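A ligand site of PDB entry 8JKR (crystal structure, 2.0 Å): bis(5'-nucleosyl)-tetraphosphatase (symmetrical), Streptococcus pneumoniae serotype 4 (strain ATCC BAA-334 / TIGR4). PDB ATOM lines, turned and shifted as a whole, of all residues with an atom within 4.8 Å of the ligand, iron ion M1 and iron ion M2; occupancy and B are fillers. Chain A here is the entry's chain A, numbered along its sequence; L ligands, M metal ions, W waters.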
ATOM      1  N   ARG A  26       3.808  15.804 -17.709  1.00  0.00           N
ATOM      2  CA  ARG A  26       5.080  15.299 -18.229  1.00  0.00           C
ATOM      3  C   ARG A  26       6.147  15.149 -17.121  1.00  0.00           C
ATOM      4  O   ARG A  26       6.916  14.165 -17.106  1.00  0.00           O
ATOM      5  CB  ARG A  26       5.573  16.184 -19.398  1.00  0.00           C
ATOM      6  CG  ARG A  26       6.783  15.657 -20.185  1.00  0.00           C
ATOM      7  CD  ARG A  26       6.621  14.211 -20.652  1.00  0.00           C
ATOM      8  NE  ARG A  26       5.494  14.073 -21.582  1.00  0.00           N
ATOM      9  CZ  ARG A  26       5.089  12.943 -22.154  1.00  0.00           C
ATOM     10  NH1 ARG A  26       4.063  12.988 -22.977  1.00  0.00           N
ATOM     11  NH2 ARG A  26       5.712  11.790 -21.931  1.00  0.00           N
ATOM     12  N   HIS A  29       5.078  12.209 -14.950  1.00  0.00           N
ATOM     13  CA  HIS A  29       5.526  11.036 -15.732  1.00  0.00           C
ATOM     14  C   HIS A  29       6.999  10.736 -15.450  1.00  0.00           C
ATOM     15  O   HIS A  29       7.343   9.615 -15.100  1.00  0.00           O
ATOM     16  CB  HIS A  29       5.273  11.235 -17.236  1.00  0.00           C
ATOM     17  CG  HIS A  29       5.999  10.262 -18.129  1.00  0.00           C
ATOM     18  ND1 HIS A  29       5.694   8.917 -18.146  1.00  0.00           N
ATOM     19  CD2 HIS A  29       6.993  10.440 -19.029  1.00  0.00           C
ATOM     20  CE1 HIS A  29       6.463   8.307 -19.033  1.00  0.00           C
ATOM     21  NE2 HIS A  29       7.265   9.200 -19.580  1.00  0.00           N
ATOM     22  N   VAL A  33       8.778   7.488 -13.835  1.00  0.00           N
ATOM     23  CA  VAL A  33       9.825   6.700 -14.506  1.00  0.00           C
ATOM     24  C   VAL A  33      11.049   6.580 -13.611  1.00  0.00           C
ATOM     25  O   VAL A  33      11.671   5.520 -13.570  1.00  0.00           O
ATOM     26  CB  VAL A  33      10.191   7.256 -15.917  1.00  0.00           C
ATOM     27  CG1 VAL A  33      11.310   6.459 -16.590  1.00  0.00           C
ATOM     28  CG2 VAL A  33       8.959   7.224 -16.845  1.00  0.00           C
ATOM     29  N   HIS A  58      14.735  11.138 -18.831  1.00  0.00           N
ATOM     30  CA  HIS A  58      14.563  10.592 -20.179  1.00  0.00           C
ATOM     31  C   HIS A  58      13.717  11.491 -21.120  1.00  0.00           C
ATOM     32  O   HIS A  58      14.004  11.565 -22.316  1.00  0.00           O
ATOM     33  CB  HIS A  58      14.003   9.180 -20.127  1.00  0.00           C
ATOM     34  CG  HIS A  58      12.522   9.163 -19.930  1.00  0.00           C
ATOM     35  ND1 HIS A  58      11.938   9.532 -18.746  1.00  0.00           N
ATOM     36  CD2 HIS A  58      11.514   8.899 -20.790  1.00  0.00           C
ATOM     37  CE1 HIS A  58      10.631   9.474 -18.870  1.00  0.00           C
ATOM     38  NE2 HIS A  58      10.353   9.078 -20.094  1.00  0.00           N
ATOM     39  N   ASP A  59      12.690  12.163 -20.567  1.00  0.00           N
ATOM     40  CA  ASP A  59      11.831  13.067 -21.336  1.00  0.00           C
ATOM     41  C   ASP A  59      12.104  14.555 -21.103  1.00  0.00           C
ATOM     42  O   ASP A  59      11.243  15.388 -21.348  1.00  0.00           O
ATOM     43  CB  ASP A  59      10.351  12.770 -21.111  1.00  0.00           C
ATOM     44  CG  ASP A  59       9.830  11.665 -22.014  1.00  0.00           C
ATOM     45  OD1 ASP A  59      10.525  11.278 -22.972  1.00  0.00           O
ATOM     46  OD2 ASP A  59       8.738  11.152 -21.725  1.00  0.00           O
ATOM     47  N   LYS A  62      11.585  16.829 -24.085  1.00  0.00           N
ATOM     48  CA  LYS A  62      10.299  16.517 -24.718  1.00  0.00           C
ATOM     49  C   LYS A  62       9.693  17.700 -25.464  1.00  0.00           C
ATOM     50  O   LYS A  62       9.133  17.528 -26.559  1.00  0.00           O
ATOM     51  CB  LYS A  62       9.310  15.977 -23.673  1.00  0.00           C
ATOM     52  CG  LYS A  62       7.968  15.472 -24.198  1.00  0.00           C
ATOM     53  CD  LYS A  62       8.071  14.238 -25.095  1.00  0.00           C
ATOM     54  CE  LYS A  62       6.707  13.608 -25.284  1.00  0.00           C
ATOM     55  NZ  LYS A  62       6.750  12.475 -26.246  1.00  0.00           N
ATOM     56  N   ASN A  88       9.094  12.702 -31.758  1.00  0.00           N
ATOM     57  CA  ASN A  88       9.130  11.326 -31.255  1.00  0.00           C
ATOM     58  C   ASN A  88      10.507  10.701 -31.291  1.00  0.00           C
ATOM     59  O   ASN A  88      10.968  10.144 -30.282  1.00  0.00           O
ATOM     60  CB  ASN A  88       8.128  10.441 -32.018  1.00  0.00           C
ATOM     61  CG  ASN A  88       6.694  10.790 -31.675  1.00  0.00           C
ATOM     62  OD1 ASN A  88       6.449  11.604 -30.806  1.00  0.00           O
ATOM     63  ND2 ASN A  88       5.752  10.138 -32.320  1.00  0.00           N
ATOM     64  N   HIS A  91      13.546  13.683 -29.419  1.00  0.00           N
ATOM     65  CA  HIS A  91      13.615  14.063 -27.989  1.00  0.00           C
ATOM     66  C   HIS A  91      14.604  13.222 -27.180  1.00  0.00           C
ATOM     67  O   HIS A  91      15.279  13.739 -26.280  1.00  0.00           O
ATOM     68  CB  HIS A  91      12.215  14.220 -27.348  1.00  0.00           C
ATOM     69  CG  HIS A  91      11.533  12.934 -26.979  1.00  0.00           C
ATOM     70  ND1 HIS A  91      10.844  12.161 -27.894  1.00  0.00           N
ATOM     71  CD2 HIS A  91      11.381  12.332 -25.778  1.00  0.00           C
ATOM     72  CE1 HIS A  91      10.311  11.125 -27.269  1.00  0.00           C
ATOM     73  NE2 HIS A  91      10.629  11.201 -25.991  1.00  0.00           N
ATOM     74  N   HIS A 117      15.554   5.580 -25.669  1.00  0.00           N
ATOM     75  CA  HIS A 117      14.408   5.210 -24.838  1.00  0.00           C
ATOM     76  C   HIS A 117      13.098   5.047 -25.621  1.00  0.00           C
ATOM     77  O   HIS A 117      12.216   4.331 -25.183  1.00  0.00           O
ATOM     78  CB  HIS A 117      14.208   6.157 -23.645  1.00  0.00           C
ATOM     79  CG  HIS A 117      13.502   7.430 -23.986  1.00  0.00           C
ATOM     80  ND1 HIS A 117      14.190   8.581 -24.348  1.00  0.00           N
ATOM     81  CD2 HIS A 117      12.192   7.758 -23.994  1.00  0.00           C
ATOM     82  CE1 HIS A 117      13.320   9.552 -24.570  1.00  0.00           C
ATOM     83  NE2 HIS A 117      12.106   9.086 -24.363  1.00  0.00           N
ATOM     84  N   THR A 118      12.990   5.717 -26.759  1.00  0.00           N
ATOM     85  CA  THR A 118      11.773   5.662 -27.597  1.00  0.00           C
ATOM     86  C   THR A 118      11.822   4.515 -28.608  1.00  0.00           C
ATOM     87  O   THR A 118      10.840   3.796 -28.776  1.00  0.00           O
ATOM     88  CB  THR A 118      11.563   6.994 -28.349  1.00  0.00           C
ATOM     89  OG1 THR A 118      11.557   8.079 -27.415  1.00  0.00           O
ATOM     90  CG2 THR A 118      10.286   6.992 -29.162  1.00  0.00           C
ATOM     91  N   VAL A 119      12.979   4.323 -29.239  1.00  0.00           N
ATOM     92  CA  VAL A 119      13.110   3.426 -30.417  1.00  0.00           C
ATOM     93  C   VAL A 119      13.886   2.134 -30.131  1.00  0.00           C
ATOM     94  O   VAL A 119      13.845   1.180 -30.930  1.00  0.00           O
ATOM     95  CB  VAL A 119      13.701   4.201 -31.628  1.00  0.00           C
ATOM     96  CG1 VAL A 119      12.839   5.420 -31.952  1.00  0.00           C
ATOM     97  CG2 VAL A 119      15.154   4.614 -31.364  1.00  0.00           C
ATOM     98  N   ASP A 135       9.665   3.482 -18.579  1.00  0.00           N
ATOM     99  CA  ASP A 135       8.917   4.511 -19.300  1.00  0.00           C
ATOM    100  C   ASP A 135       7.467   4.056 -19.544  1.00  0.00           C
ATOM    101  O   ASP A 135       6.492   4.807 -19.358  1.00  0.00           O
ATOM    102  CB  ASP A 135       9.646   4.810 -20.621  1.00  0.00           C
ATOM    103  CG  ASP A 135       9.034   5.962 -21.393  1.00  0.00           C
ATOM    104  OD1 ASP A 135       8.402   6.836 -20.781  1.00  0.00           O
ATOM    105  OD2 ASP A 135       9.198   5.976 -22.636  1.00  0.00           O
ATOM    106  N   GLU A 164       6.623  -4.466 -25.225  1.00  0.00           N
ATOM    107  CA  GLU A 164       6.479  -3.025 -25.482  1.00  0.00           C
ATOM    108  C   GLU A 164       6.721  -2.727 -26.965  1.00  0.00           C
ATOM    109  O   GLU A 164       5.890  -2.058 -27.591  1.00  0.00           O
ATOM    110  CB  GLU A 164       7.438  -2.202 -24.633  1.00  0.00           C
ATOM    111  CG  GLU A 164       7.339  -0.717 -24.971  1.00  0.00           C
ATOM    112  CD  GLU A 164       8.219   0.186 -24.126  1.00  0.00           C
ATOM    113  OE1 GLU A 164       8.826  -0.269 -23.112  1.00  0.00           O
ATOM    114  OE2 GLU A 164       8.298   1.390 -24.485  1.00  0.00           O
ATOM    115  N   THR A 168       4.062  -1.204 -29.752  1.00  0.00           N
ATOM    116  CA  THR A 168       4.329   0.100 -30.400  1.00  0.00           C
ATOM    117  C   THR A 168       4.269  -0.008 -31.930  1.00  0.00           C
ATOM    118  O   THR A 168       3.550   0.766 -32.580  1.00  0.00           O
ATOM    119  CB  THR A 168       5.691   0.657 -29.928  1.00  0.00           C
ATOM    120  OG1 THR A 168       5.595   0.921 -28.530  1.00  0.00           O
ATOM    121  CG2 THR A 168       6.082   1.974 -30.650  1.00  0.00           C
ATOM    122  N   TYR A 171       0.680  -0.612 -32.895  1.00  0.00           N
ATOM    123  CA  TYR A 171      -0.101   0.625 -32.755  1.00  0.00           C
ATOM    124  C   TYR A 171       0.227   1.661 -33.856  1.00  0.00           C
ATOM    125  O   TYR A 171      -0.695   2.255 -34.418  1.00  0.00           O
ATOM    126  CB  TYR A 171       0.039   1.209 -31.353  1.00  0.00           C
ATOM    127  CG  TYR A 171      -0.549   2.602 -31.189  1.00  0.00           C
ATOM    128  CD1 TYR A 171      -1.918   2.792 -30.950  1.00  0.00           C
ATOM    129  CD2 TYR A 171       0.285   3.733 -31.249  1.00  0.00           C
ATOM    130  CE1 TYR A 171      -2.449   4.069 -30.780  1.00  0.00           C
ATOM    131  CE2 TYR A 171      -0.241   5.006 -31.092  1.00  0.00           C
ATOM    132  CZ  TYR A 171      -1.597   5.172 -30.857  1.00  0.00           C
ATOM    133  OH  TYR A 171      -2.088   6.456 -30.706  1.00  0.00           O
ATOM    134  N   LEU A 172       1.511   1.850 -34.165  1.00  0.00           N
ATOM    135  CA  LEU A 172       1.919   2.798 -35.204  1.00  0.00           C
ATOM    136  C   LEU A 172       1.400   2.378 -36.576  1.00  0.00           C
ATOM    137  O   LEU A 172       0.927   3.249 -37.314  1.00  0.00           O
ATOM    138  CB  LEU A 172       3.436   3.007 -35.211  1.00  0.00           C
ATOM    139  CG  LEU A 172       4.001   3.725 -33.979  1.00  0.00           C
ATOM    140  CD1 LEU A 172       5.523   3.746 -34.059  1.00  0.00           C
ATOM    141  CD2 LEU A 172       3.433   5.139 -33.829  1.00  0.00           C
ATOM    142  N   PRO A 178       4.525   6.791 -39.571  1.00  0.00           N
ATOM    143  CA  PRO A 178       5.825   6.232 -39.965  1.00  0.00           C
ATOM    144  C   PRO A 178       6.477   5.551 -38.757  1.00  0.00           C
ATOM    145  O   PRO A 178       6.188   5.914 -37.607  1.00  0.00           O
ATOM    146  CB  PRO A 178       6.658   7.449 -40.406  1.00  0.00           C
ATOM    147  CG  PRO A 178       5.670   8.541 -40.658  1.00  0.00           C
ATOM    148  CD  PRO A 178       4.480   8.266 -39.760  1.00  0.00           C
ATOM    149  N   ILE A 179       7.304   4.555 -39.028  1.00  0.00           N
ATOM    150  CA  ILE A 179       8.017   3.814 -38.000  1.00  0.00           C
ATOM    151  C   ILE A 179       9.515   3.959 -38.232  1.00  0.00           C
ATOM    152  O   ILE A 179      10.043   3.554 -39.280  1.00  0.00           O
ATOM    153  CB  ILE A 179       7.609   2.316 -38.016  1.00  0.00           C
ATOM    154  CG1 ILE A 179       6.124   2.143 -37.623  1.00  0.00           C
ATOM    155  CG2 ILE A 179       8.519   1.494 -37.085  1.00  0.00           C
ATOM    156  CD1 ILE A 179       5.522   0.807 -38.029  1.00  0.00           C
ATOM    157  N   TYR A 180      10.214   4.514 -37.239  1.00  0.00           N
ATOM    158  CA  TYR A 180      11.651   4.701 -37.335  1.00  0.00           C
ATOM    159  C   TYR A 180      12.327   3.345 -37.529  1.00  0.00           C
ATOM    160  O   TYR A 180      12.023   2.405 -36.796  1.00  0.00           O
ATOM    161  CB  TYR A 180      12.195   5.416 -36.093  1.00  0.00           C
ATOM    162  CG  TYR A 180      13.578   5.988 -36.287  1.00  0.00           C
ATOM    163  CD1 TYR A 180      13.818   7.000 -37.227  1.00  0.00           C
ATOM    164  CD2 TYR A 180      14.660   5.501 -35.551  1.00  0.00           C
ATOM    165  CE1 TYR A 180      15.086   7.517 -37.411  1.00  0.00           C
ATOM    166  CE2 TYR A 180      15.940   6.002 -35.750  1.00  0.00           C
ATOM    167  CZ  TYR A 180      16.147   7.018 -36.673  1.00  0.00           C
ATOM    168  OH  TYR A 180      17.416   7.519 -36.852  1.00  0.00           O
ATOM    169  N   THR A 183      13.593   1.252 -34.646  1.00  0.00           N
ATOM    170  CA  THR A 183      12.515   0.582 -33.889  1.00  0.00           C
ATOM    171  C   THR A 183      12.307  -0.846 -34.370  1.00  0.00           C
ATOM    172  O   THR A 183      12.099  -1.757 -33.545  1.00  0.00           O
ATOM    173  CB  THR A 183      11.200   1.374 -33.929  1.00  0.00           C
ATOM    174  OG1 THR A 183      11.444   2.675 -33.393  1.00  0.00           O
ATOM    175  CG2 THR A 183      10.091   0.709 -33.107  1.00  0.00           C
HETATM  176  N1  LIG L   1       7.029   6.399 -31.686  1.00  0.00           N
HETATM  177  C1  LIG L   1       7.294   6.729 -33.037  1.00  0.00           C
HETATM  178  N2  LIG L   1       8.169   6.018 -33.755  1.00  0.00           N
HETATM  179  C2  LIG L   1       8.820   4.993 -33.182  1.00  0.00           C
HETATM  180  C3  LIG L   1       8.568   4.639 -31.835  1.00  0.00           C
HETATM  181  C4  LIG L   1       7.656   5.380 -31.085  1.00  0.00           C
HETATM  182  O1  LIG L   1       6.686   7.689 -33.569  1.00  0.00           O
HETATM  183  O2  LIG L   1       9.631   4.387 -33.905  1.00  0.00           O
HETATM  184  C5  LIG L   1       6.038   7.155 -30.939  1.00  0.00           C
HETATM  185  C6  LIG L   1       5.330   6.289 -29.896  1.00  0.00           C
HETATM  186  O3  LIG L   1       4.003   5.992 -30.315  1.00  0.00           O
HETATM  187  C7  LIG L   1       5.361   7.140 -28.644  1.00  0.00           C
HETATM  188  C8  LIG L   1       6.135   8.396 -28.978  1.00  0.00           C
HETATM  189  O4  LIG L   1       4.062   7.583 -28.235  1.00  0.00           O
HETATM  190  O5  LIG L   1       6.663   8.263 -30.301  1.00  0.00           O
HETATM  191  C9  LIG L   1       7.229   8.730 -27.964  1.00  0.00           C
HETATM  192  O6  LIG L   1       7.681   7.510 -27.399  1.00  0.00           O
HETATM  193  P1  LIG L   1       8.199   7.390 -25.900  1.00  0.00           P
HETATM  194  O7  LIG L   1       9.447   8.245 -25.986  1.00  0.00           O
HETATM  195  O8  LIG L   1       7.014   7.885 -25.125  1.00  0.00           O
HETATM  196  O9  LIG L   1       8.413   5.904 -25.729  1.00  0.00           O
HETATM  197 FE    FE M   1      10.056   9.758 -24.448  1.00  0.00          FE
HETATM  198 FE    FE M   2       8.480   8.955 -21.188  1.00  0.00          FE
HETATM  199  O   HOH W   1       8.014   4.307 -27.945  1.00  0.00           O
HETATM  200  O   HOH W   2       9.180   8.711 -22.953  1.00  0.00           O
HETATM  201  O   HOH W   3       9.771   3.934 -24.387  1.00  0.00           O
HETATM  202  O   HOH W   4       6.378   4.830 -23.507  1.00  0.00           O
HETATM  203  O   HOH W   5       6.661   8.628 -22.246  1.00  0.00           O
HETATM  204  O   HOH W   6       8.163  10.458 -24.341  1.00  0.00           O
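Merely in contact with the ligand: Val 119 (3.9 Å), Thr 168 (3.8 Å) and Leu 172 (3.5 Å).
Hydrophobic or aromatic side chains within 4 Å of the ligand: His 91, His 117, Val 119, Leu 172 and Tyr 180.
Ten residues have an atom within 4 Å of the ligand: Asn 88, His 91, His 117, Thr 118, Val 119, Asp 135, Thr 168, Leu 172, Tyr 180 and Thr 183.
The side-chain hydroxyl (OG1) of Thr 183 is in hydrogen-bond range of an oxygen (O2) of the ligand, at 2.5 Å.
OG1 of Thr 118 sits close to O7 of the ligand, 2.6 Å away.
An oxygen (O5) of the ligand lies close to the side-chain amide nitrogen (ND2) of Asn 88 (2.9 Å).
An oxygen (O2) of the ligand is in hydrogen-bond range of the backbone NH (N) of Tyr 180.
Iron ion M2 is bound by water W2 (1.9 Å), a ring nitrogen (NE2) of His 29 (2.0 Å), water W5 (2.1 Å), the side-chain carboxylate (OD1) of Asp 135 (2.2 Å), a ring nitrogen (NE2) of His 58 (2.2 Å) and the side-chain carboxylate (OD2) of Asp 59 (2.3 Å).
NE2 of His 117 lies close to OG1 of Thr 118.
The side-chain carboxylate (OD2) of Asp 59 sits close to the guanidinium group (NH2) of Arg 26, at 3.1 Å.
The backbone carbonyl oxygen of Asn 88 lies within hydrogen-bond range of a ring nitrogen (ND1) of His 91.
OG1 of Thr 183 sits close to O of Tyr 180 (3.5 Å).
OG1 of Thr 168 lies within hydrogen-bond range of O of Glu 164 (3.1 Å).
Along chain A the residues within 4 Å of iron ion M2 span positions 29 to 135.
Water W6 bridges an oxygen (O8) of the ligand (2.9 Å) and the side-chain amino group of Lys 62 (3.1 Å).
Water W2 bridges OD2 of Asp 135 and O8 of the ligand.
Water W5 bridges O8 of the ligand (3.0 Å) and NH2 of Arg 26 (3.3 Å).
Water W1 lies within hydrogen-bond range of an oxygen (O9) of the ligand (2.8 Å) and the backbone carbonyl oxygen of Thr 118 (3.0 Å).
Water W4 lies within hydrogen-bond range of OD2 of Asp 135 and O9 of the ligand.
Iron ion M1 is bound by water W6 (2.0 Å), water W2 (2.0 Å), a ring nitrogen (NE2) of His 117 (2.2 Å), the side-chain carboxylate of Asp 59 (2.2 Å), a ring nitrogen (NE2) of His 91 (2.2 Å) and an oxygen (O7) of the ligand (2.2 Å).
Iron ion M1 has six donor atoms within binding distance.
Merely in contact with iron ion M1: Thr 118 (3.7 Å).
Four residues have an atom within 4 Å of iron ion M1: Asp 59, His 91, His 117 and Thr 118.
The nearest printed residue that does not touch iron ion M1 is His 58 (4.03 Å).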
